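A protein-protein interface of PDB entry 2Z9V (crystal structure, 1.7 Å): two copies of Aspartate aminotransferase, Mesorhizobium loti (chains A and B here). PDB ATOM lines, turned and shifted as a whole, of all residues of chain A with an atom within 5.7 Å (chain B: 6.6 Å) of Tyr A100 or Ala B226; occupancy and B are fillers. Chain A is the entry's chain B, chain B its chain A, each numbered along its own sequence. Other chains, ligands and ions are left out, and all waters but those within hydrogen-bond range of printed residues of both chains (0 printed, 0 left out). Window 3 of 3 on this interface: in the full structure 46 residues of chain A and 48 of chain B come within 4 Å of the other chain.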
ATOM      1  N   GLU A  73      23.228 -20.107  19.151  1.00  0.00           N
ATOM      2  CA  GLU A  73      23.445 -20.630  20.488  1.00  0.00           C
ATOM      3  C   GLU A  73      24.514 -21.747  20.510  1.00  0.00           C
ATOM      4  O   GLU A  73      25.392 -21.768  21.374  1.00  0.00           O
ATOM      5  CB  GLU A  73      22.140 -21.166  21.075  1.00  0.00           C
ATOM      6  CG  GLU A  73      22.315 -21.603  22.510  1.00  0.00           C
ATOM      7  CD  GLU A  73      21.049 -22.207  23.091  1.00  0.00           C
ATOM      8  OE1 GLU A  73      20.046 -22.337  22.358  1.00  0.00           O
ATOM      9  OE2 GLU A  73      21.076 -22.548  24.290  1.00  0.00           O
ATOM     10  N   LYS A  96      23.444  -7.267  19.817  1.00  0.00           N
ATOM     11  CA  LYS A  96      23.485  -7.132  21.269  1.00  0.00           C
ATOM     12  C   LYS A  96      23.126  -8.467  21.927  1.00  0.00           C
ATOM     13  O   LYS A  96      23.775  -8.893  22.875  1.00  0.00           O
ATOM     14  CB  LYS A  96      22.525  -6.025  21.730  1.00  0.00           C
ATOM     15  CG  LYS A  96      22.532  -5.738  23.221  1.00  0.00           C
ATOM     16  CD  LYS A  96      23.834  -5.097  23.689  1.00  0.00           C
ATOM     17  CE  LYS A  96      23.796  -4.826  25.192  1.00  0.00           C
ATOM     18  NZ  LYS A  96      25.123  -4.343  25.728  1.00  0.00           N
ATOM     19  N   GLY A  97      22.105  -9.123  21.395  1.00  0.00           N
ATOM     20  CA  GLY A  97      21.637 -10.396  21.932  1.00  0.00           C
ATOM     21  C   GLY A  97      22.729 -11.454  21.936  1.00  0.00           C
ATOM     22  O   GLY A  97      22.786 -12.293  22.846  1.00  0.00           O
ATOM     23  N   PHE A  98      23.594 -11.442  20.928  1.00  0.00           N
ATOM     24  CA  PHE A  98      24.614 -12.487  20.879  1.00  0.00           C
ATOM     25  C   PHE A  98      25.548 -12.367  22.085  1.00  0.00           C
ATOM     26  O   PHE A  98      26.013 -13.376  22.603  1.00  0.00           O
ATOM     27  CB  PHE A  98      25.428 -12.476  19.597  1.00  0.00           C
ATOM     28  CG  PHE A  98      26.295 -13.690  19.467  1.00  0.00           C
ATOM     29  CD1 PHE A  98      27.593 -13.688  19.958  1.00  0.00           C
ATOM     30  CD2 PHE A  98      25.778 -14.855  18.918  1.00  0.00           C
ATOM     31  CE1 PHE A  98      28.380 -14.839  19.888  1.00  0.00           C
ATOM     32  CE2 PHE A  98      26.552 -16.013  18.843  1.00  0.00           C
ATOM     33  CZ  PHE A  98      27.856 -16.003  19.323  1.00  0.00           C
ATOM     34  N   GLY A  99      25.802 -11.138  22.535  1.00  0.00           N
ATOM     35  CA  GLY A  99      26.623 -10.903  23.727  1.00  0.00           C
ATOM     36  C   GLY A  99      26.139 -11.630  24.973  1.00  0.00           C
ATOM     37  O   GLY A  99      26.951 -12.026  25.810  1.00  0.00           O
ATOM     38  N   TYR A 100      24.819 -11.794  25.096  1.00  0.00           N
ATOM     39  CA  TYR A 100      24.208 -12.534  26.209  1.00  0.00           C
ATOM     40  C   TYR A 100      24.631 -14.001  26.199  1.00  0.00           C
ATOM     41  O   TYR A 100      24.943 -14.584  27.238  1.00  0.00           O
ATOM     42  CB  TYR A 100      22.673 -12.446  26.153  1.00  0.00           C
ATOM     43  CG  TYR A 100      21.983 -13.043  27.368  1.00  0.00           C
ATOM     44  CD1 TYR A 100      21.479 -14.347  27.346  1.00  0.00           C
ATOM     45  CD2 TYR A 100      21.828 -12.299  28.538  1.00  0.00           C
ATOM     46  CE1 TYR A 100      20.846 -14.890  28.459  1.00  0.00           C
ATOM     47  CE2 TYR A 100      21.201 -12.832  29.657  1.00  0.00           C
ATOM     48  CZ  TYR A 100      20.712 -14.122  29.613  1.00  0.00           C
ATOM     49  OH  TYR A 100      20.093 -14.649  30.723  1.00  0.00           O
ATOM     50  N   TRP A 101      24.627 -14.606  25.014  1.00  0.00           N
ATOM     51  CA  TRP A 101      25.121 -15.975  24.886  1.00  0.00           C
ATOM     52  C   TRP A 101      26.629 -16.057  25.079  1.00  0.00           C
ATOM     53  O   TRP A 101      27.123 -17.010  25.683  1.00  0.00           O
ATOM     54  CB  TRP A 101      24.718 -16.592  23.555  1.00  0.00           C
ATOM     55  CG  TRP A 101      23.299 -17.122  23.559  1.00  0.00           C
ATOM     56  CD1 TRP A 101      22.599 -17.616  24.636  1.00  0.00           C
ATOM     57  CD2 TRP A 101      22.440 -17.259  22.427  1.00  0.00           C
ATOM     58  NE1 TRP A 101      21.354 -18.038  24.238  1.00  0.00           N
ATOM     59  CE2 TRP A 101      21.228 -17.835  22.889  1.00  0.00           C
ATOM     60  CE3 TRP A 101      22.569 -16.951  21.066  1.00  0.00           C
ATOM     61  CZ2 TRP A 101      20.147 -18.096  22.038  1.00  0.00           C
ATOM     62  CZ3 TRP A 101      21.488 -17.220  20.211  1.00  0.00           C
ATOM     63  CH2 TRP A 101      20.292 -17.782  20.711  1.00  0.00           C
ATOM     64  N   ALA A 102      27.373 -15.068  24.567  1.00  0.00           N
ATOM     65  CA  ALA A 102      28.818 -15.049  24.799  1.00  0.00           C
ATOM     66  C   ALA A 102      29.091 -15.064  26.305  1.00  0.00           C
ATOM     67  O   ALA A 102      29.882 -15.869  26.775  1.00  0.00           O
ATOM     68  CB  ALA A 102      29.476 -13.825  24.135  1.00  0.00           C
ATOM     69  N   LYS A 103      28.400 -14.196  27.051  1.00  0.00           N
ATOM     70  CA  LYS A 103      28.607 -14.084  28.493  1.00  0.00           C
ATOM     71  C   LYS A 103      28.209 -15.352  29.265  1.00  0.00           C
ATOM     72  O   LYS A 103      28.760 -15.648  30.331  1.00  0.00           O
ATOM     73  CB  LYS A 103      27.842 -12.880  29.040  1.00  0.00           C
ATOM     74  CG  LYS A 103      28.227 -12.510  30.469  1.00  0.00           C
ATOM     75  CD  LYS A 103      29.592 -11.845  30.547  1.00  0.00           C
ATOM     76  CE  LYS A 103      29.949 -11.517  31.987  1.00  0.00           C
ATOM     77  NZ  LYS A 103      29.036 -10.461  32.531  1.00  0.00           N
ATOM     78  N   ARG A 104      27.286 -16.118  28.703  1.00  0.00           N
ATOM     79  CA  ARG A 104      26.917 -17.402  29.296  1.00  0.00           C
ATOM     80  C   ARG A 104      28.102 -18.384  29.251  1.00  0.00           C
ATOM     81  O   ARG A 104      28.261 -19.234  30.153  1.00  0.00           O
ATOM     82  CB  ARG A 104      25.696 -17.985  28.583  1.00  0.00           C
ATOM     83  CG  ARG A 104      25.396 -19.430  28.942  1.00  0.00           C
ATOM     84  CD  ARG A 104      24.070 -19.876  28.341  1.00  0.00           C
ATOM     85  NE  ARG A 104      22.975 -19.145  28.993  1.00  0.00           N
ATOM     86  CZ  ARG A 104      21.710 -19.096  28.565  1.00  0.00           C
ATOM     87  NH1 ARG A 104      21.329 -19.744  27.462  1.00  0.00           N
ATOM     88  NH2 ARG A 104      20.824 -18.381  29.260  1.00  0.00           N
ATOM     89  N   TYR A 105      28.948 -18.241  28.230  1.00  0.00           N
ATOM     90  CA  TYR A 105      30.012 -19.224  27.980  1.00  0.00           C
ATOM     91  C   TYR A 105      31.434 -18.743  28.303  1.00  0.00           C
ATOM     92  O   TYR A 105      32.377 -19.552  28.388  1.00  0.00           O
ATOM     93  CB  TYR A 105      29.877 -19.794  26.564  1.00  0.00           C
ATOM     94  CG  TYR A 105      28.622 -20.630  26.451  1.00  0.00           C
ATOM     95  CD1 TYR A 105      28.535 -21.869  27.101  1.00  0.00           C
ATOM     96  CD2 TYR A 105      27.505 -20.164  25.750  1.00  0.00           C
ATOM     97  CE1 TYR A 105      27.369 -22.632  27.031  1.00  0.00           C
ATOM     98  CE2 TYR A 105      26.325 -20.922  25.675  1.00  0.00           C
ATOM     99  CZ  TYR A 105      26.277 -22.156  26.321  1.00  0.00           C
ATOM    100  OH  TYR A 105      25.151 -22.951  26.251  1.00  0.00           O
ATOM    101  N   LEU A 109      33.892 -10.358  28.484  1.00  0.00           N
ATOM    102  CA  LEU A 109      33.172  -9.764  27.366  1.00  0.00           C
ATOM    103  C   LEU A 109      33.519  -8.292  27.231  1.00  0.00           C
ATOM    104  O   LEU A 109      33.311  -7.496  28.162  1.00  0.00           O
ATOM    105  CB  LEU A 109      31.648  -9.903  27.556  1.00  0.00           C
ATOM    106  CG  LEU A 109      30.758  -9.329  26.434  1.00  0.00           C
ATOM    107  CD1 LEU A 109      30.998 -10.095  25.111  1.00  0.00           C
ATOM    108  CD2 LEU A 109      29.270  -9.374  26.833  1.00  0.00           C
ATOM    109  N   PRO B 224      16.884 -24.535  31.558  1.00  0.00           N
ATOM    110  CA  PRO B 224      17.224 -23.663  30.427  1.00  0.00           C
ATOM    111  C   PRO B 224      16.218 -22.525  30.170  1.00  0.00           C
ATOM    112  O   PRO B 224      14.991 -22.728  30.176  1.00  0.00           O
ATOM    113  CB  PRO B 224      17.298 -24.633  29.245  1.00  0.00           C
ATOM    114  CG  PRO B 224      17.752 -25.929  29.877  1.00  0.00           C
ATOM    115  CD  PRO B 224      16.999 -25.966  31.212  1.00  0.00           C
ATOM    116  N   ARG B 225      16.776 -21.325  29.978  1.00  0.00           N
ATOM    117  CA  ARG B 225      16.044 -20.121  29.629  1.00  0.00           C
ATOM    118  C   ARG B 225      16.912 -19.413  28.592  1.00  0.00           C
ATOM    119  O   ARG B 225      18.142 -19.561  28.635  1.00  0.00           O
ATOM    120  CB  ARG B 225      15.842 -19.247  30.863  1.00  0.00           C
ATOM    121  CG  ARG B 225      14.821 -19.825  31.858  1.00  0.00           C
ATOM    122  CD  ARG B 225      14.804 -19.063  33.178  1.00  0.00           C
ATOM    123  NE  ARG B 225      13.792 -19.622  34.081  1.00  0.00           N
ATOM    124  CZ  ARG B 225      14.016 -20.572  34.986  1.00  0.00           C
ATOM    125  NH1 ARG B 225      13.012 -21.003  35.745  1.00  0.00           N
ATOM    126  NH2 ARG B 225      15.223 -21.102  35.142  1.00  0.00           N
ATOM    127  N   ALA B 226      16.278 -18.685  27.664  1.00  0.00           N
ATOM    128  CA  ALA B 226      16.994 -18.088  26.517  1.00  0.00           C
ATOM    129  C   ALA B 226      17.827 -19.169  25.822  1.00  0.00           C
ATOM    130  O   ALA B 226      19.051 -19.040  25.654  1.00  0.00           O
ATOM    131  CB  ALA B 226      17.875 -16.927  26.990  1.00  0.00           C
ATOM    132  N   SER B 227      17.153 -20.248  25.429  1.00  0.00           N
ATOM    133  CA  SER B 227      17.827 -21.442  24.937  1.00  0.00           C
ATOM    134  C   SER B 227      16.867 -22.291  24.125  1.00  0.00           C
ATOM    135  O   SER B 227      15.688 -22.370  24.451  1.00  0.00           O
ATOM    136  CB  SER B 227      18.352 -22.278  26.110  1.00  0.00           C
ATOM    137  OG  SER B 227      18.967 -23.470  25.644  1.00  0.00           O
ATOM    138  N   MET B 228      17.379 -22.948  23.090  1.00  0.00           N
ATOM    139  CA  MET B 228      16.605 -23.951  22.353  1.00  0.00           C
ATOM    140  C   MET B 228      16.085 -25.029  23.297  1.00  0.00           C
ATOM    141  O   MET B 228      15.042 -25.634  23.035  1.00  0.00           O
ATOM    142  CB  MET B 228      17.452 -24.628  21.267  1.00  0.00           C
ATOM    143  CG  MET B 228      16.619 -25.380  20.250  1.00  0.00           C
ATOM    144  SD  MET B 228      16.203 -24.379  18.812  1.00  0.00           S
ATOM    145  CE  MET B 228      16.368 -22.715  19.413  1.00  0.00           C
ATOM    146  N   LEU B 229      16.827 -25.273  24.379  1.00  0.00           N
ATOM    147  CA  LEU B 229      16.436 -26.270  25.368  1.00  0.00           C
ATOM    148  C   LEU B 229      15.380 -25.786  26.371  1.00  0.00           C
ATOM    149  O   LEU B 229      14.996 -26.539  27.268  1.00  0.00           O
ATOM    150  CB  LEU B 229      17.669 -26.794  26.123  1.00  0.00           C
ATOM    151  CG  LEU B 229      18.775 -27.459  25.302  1.00  0.00           C
ATOM    152  CD1 LEU B 229      19.867 -27.967  26.236  1.00  0.00           C
ATOM    153  CD2 LEU B 229      18.220 -28.580  24.464  1.00  0.00           C
ATOM    154  N   SER B 230      14.907 -24.555  26.239  1.00  0.00           N
ATOM    155  CA  SER B 230      13.955 -24.017  27.234  1.00  0.00           C
ATOM    156  C   SER B 230      12.537 -24.524  26.998  1.00  0.00           C
ATOM    157  O   SER B 230      11.982 -24.365  25.916  1.00  0.00           O
ATOM    158  CB  SER B 230      13.951 -22.489  27.231  1.00  0.00           C
ATOM    159  OG  SER B 230      13.147 -21.986  28.301  1.00  0.00           O
ATOM    160  N   ASP B 233      10.350 -20.995  28.743  1.00  0.00           N
ATOM    161  CA  ASP B 233      10.167 -19.828  27.882  1.00  0.00           C
ATOM    162  C   ASP B 233       8.937 -19.942  26.968  1.00  0.00           C
ATOM    163  O   ASP B 233       8.405 -18.931  26.532  1.00  0.00           O
ATOM    164  CB  ASP B 233      11.412 -19.562  27.021  1.00  0.00           C
ATOM    165  CG  ASP B 233      12.582 -18.977  27.818  1.00  0.00           C
ATOM    166  OD1 ASP B 233      13.636 -18.777  27.193  1.00  0.00           O
ATOM    167  OD2 ASP B 233      12.469 -18.727  29.043  1.00  0.00           O
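Hydrophobic or aromatic side chains of chain B within 4 Å of the printed part of chain A: Ala B226 and Met B228.
Of the printed residues of chain B, Glu A73 touches Ser B227 (2.7 Å) and Met B228 (2.8 Å).
Of the printed residues of chain B, Tyr A100 touches Ala B226 (3.9 Å).
Printed residues of chain B within 4 Å of Arg A104: Arg B225 and Ala B226.
Printed residues of chain A within 4 Å of Arg B225: Arg A104 (3.0 Å).
Printed residues of chain A within 4 Å of Met B228: Glu A73.
The nearest printed residue of chain B that does not touch Tyr A100 is Arg B225 (5.4 Å).
The nearest printed residue of chain A that does not touch Ala B226 is Glu A73 (4.3 Å).
The nearest printed residue of chain A that does not touch Met B228 is Trp A101 (5.7 Å).
The backbone carbonyl oxygen (O) of Arg B225 lies within hydrogen-bond range of the guanidinium group (NH2) of Arg A104 (3.0 Å).
O of Ala B226 is in hydrogen-bond range of NE1 of Trp A101, 2.9 Å away.
The backbone carbonyl oxygen (O) of Ala B226 lies within hydrogen-bond range of the guanidinium group (NH1) of Arg A104 (3.0 Å).
The side-chain carboxylate (OE2) of Glu A73 sits at hydrogen-bond distance from the side-chain hydroxyl (OG) of Ser B227 (2.7 Å).
The backbone NH (N) of Met B228 is in hydrogen-bond range of the side-chain carboxylate (OE1) of Glu A73, 2.8 Å away.
The backbone NH (N) of Ala B226 lies within hydrogen-bond range of the side-chain carboxylate (OD1) of Asp B233, at 2.7 Å.
The side-chain hydroxyl (OG) of Ser B227 sits close to the backbone NH (N) of Leu B229 (3.1 Å).
No position is printed for both chains.
Among the printed residues, pairs that only touch across the chains: Tyr A100 with Ala B226 (3.9 Å).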
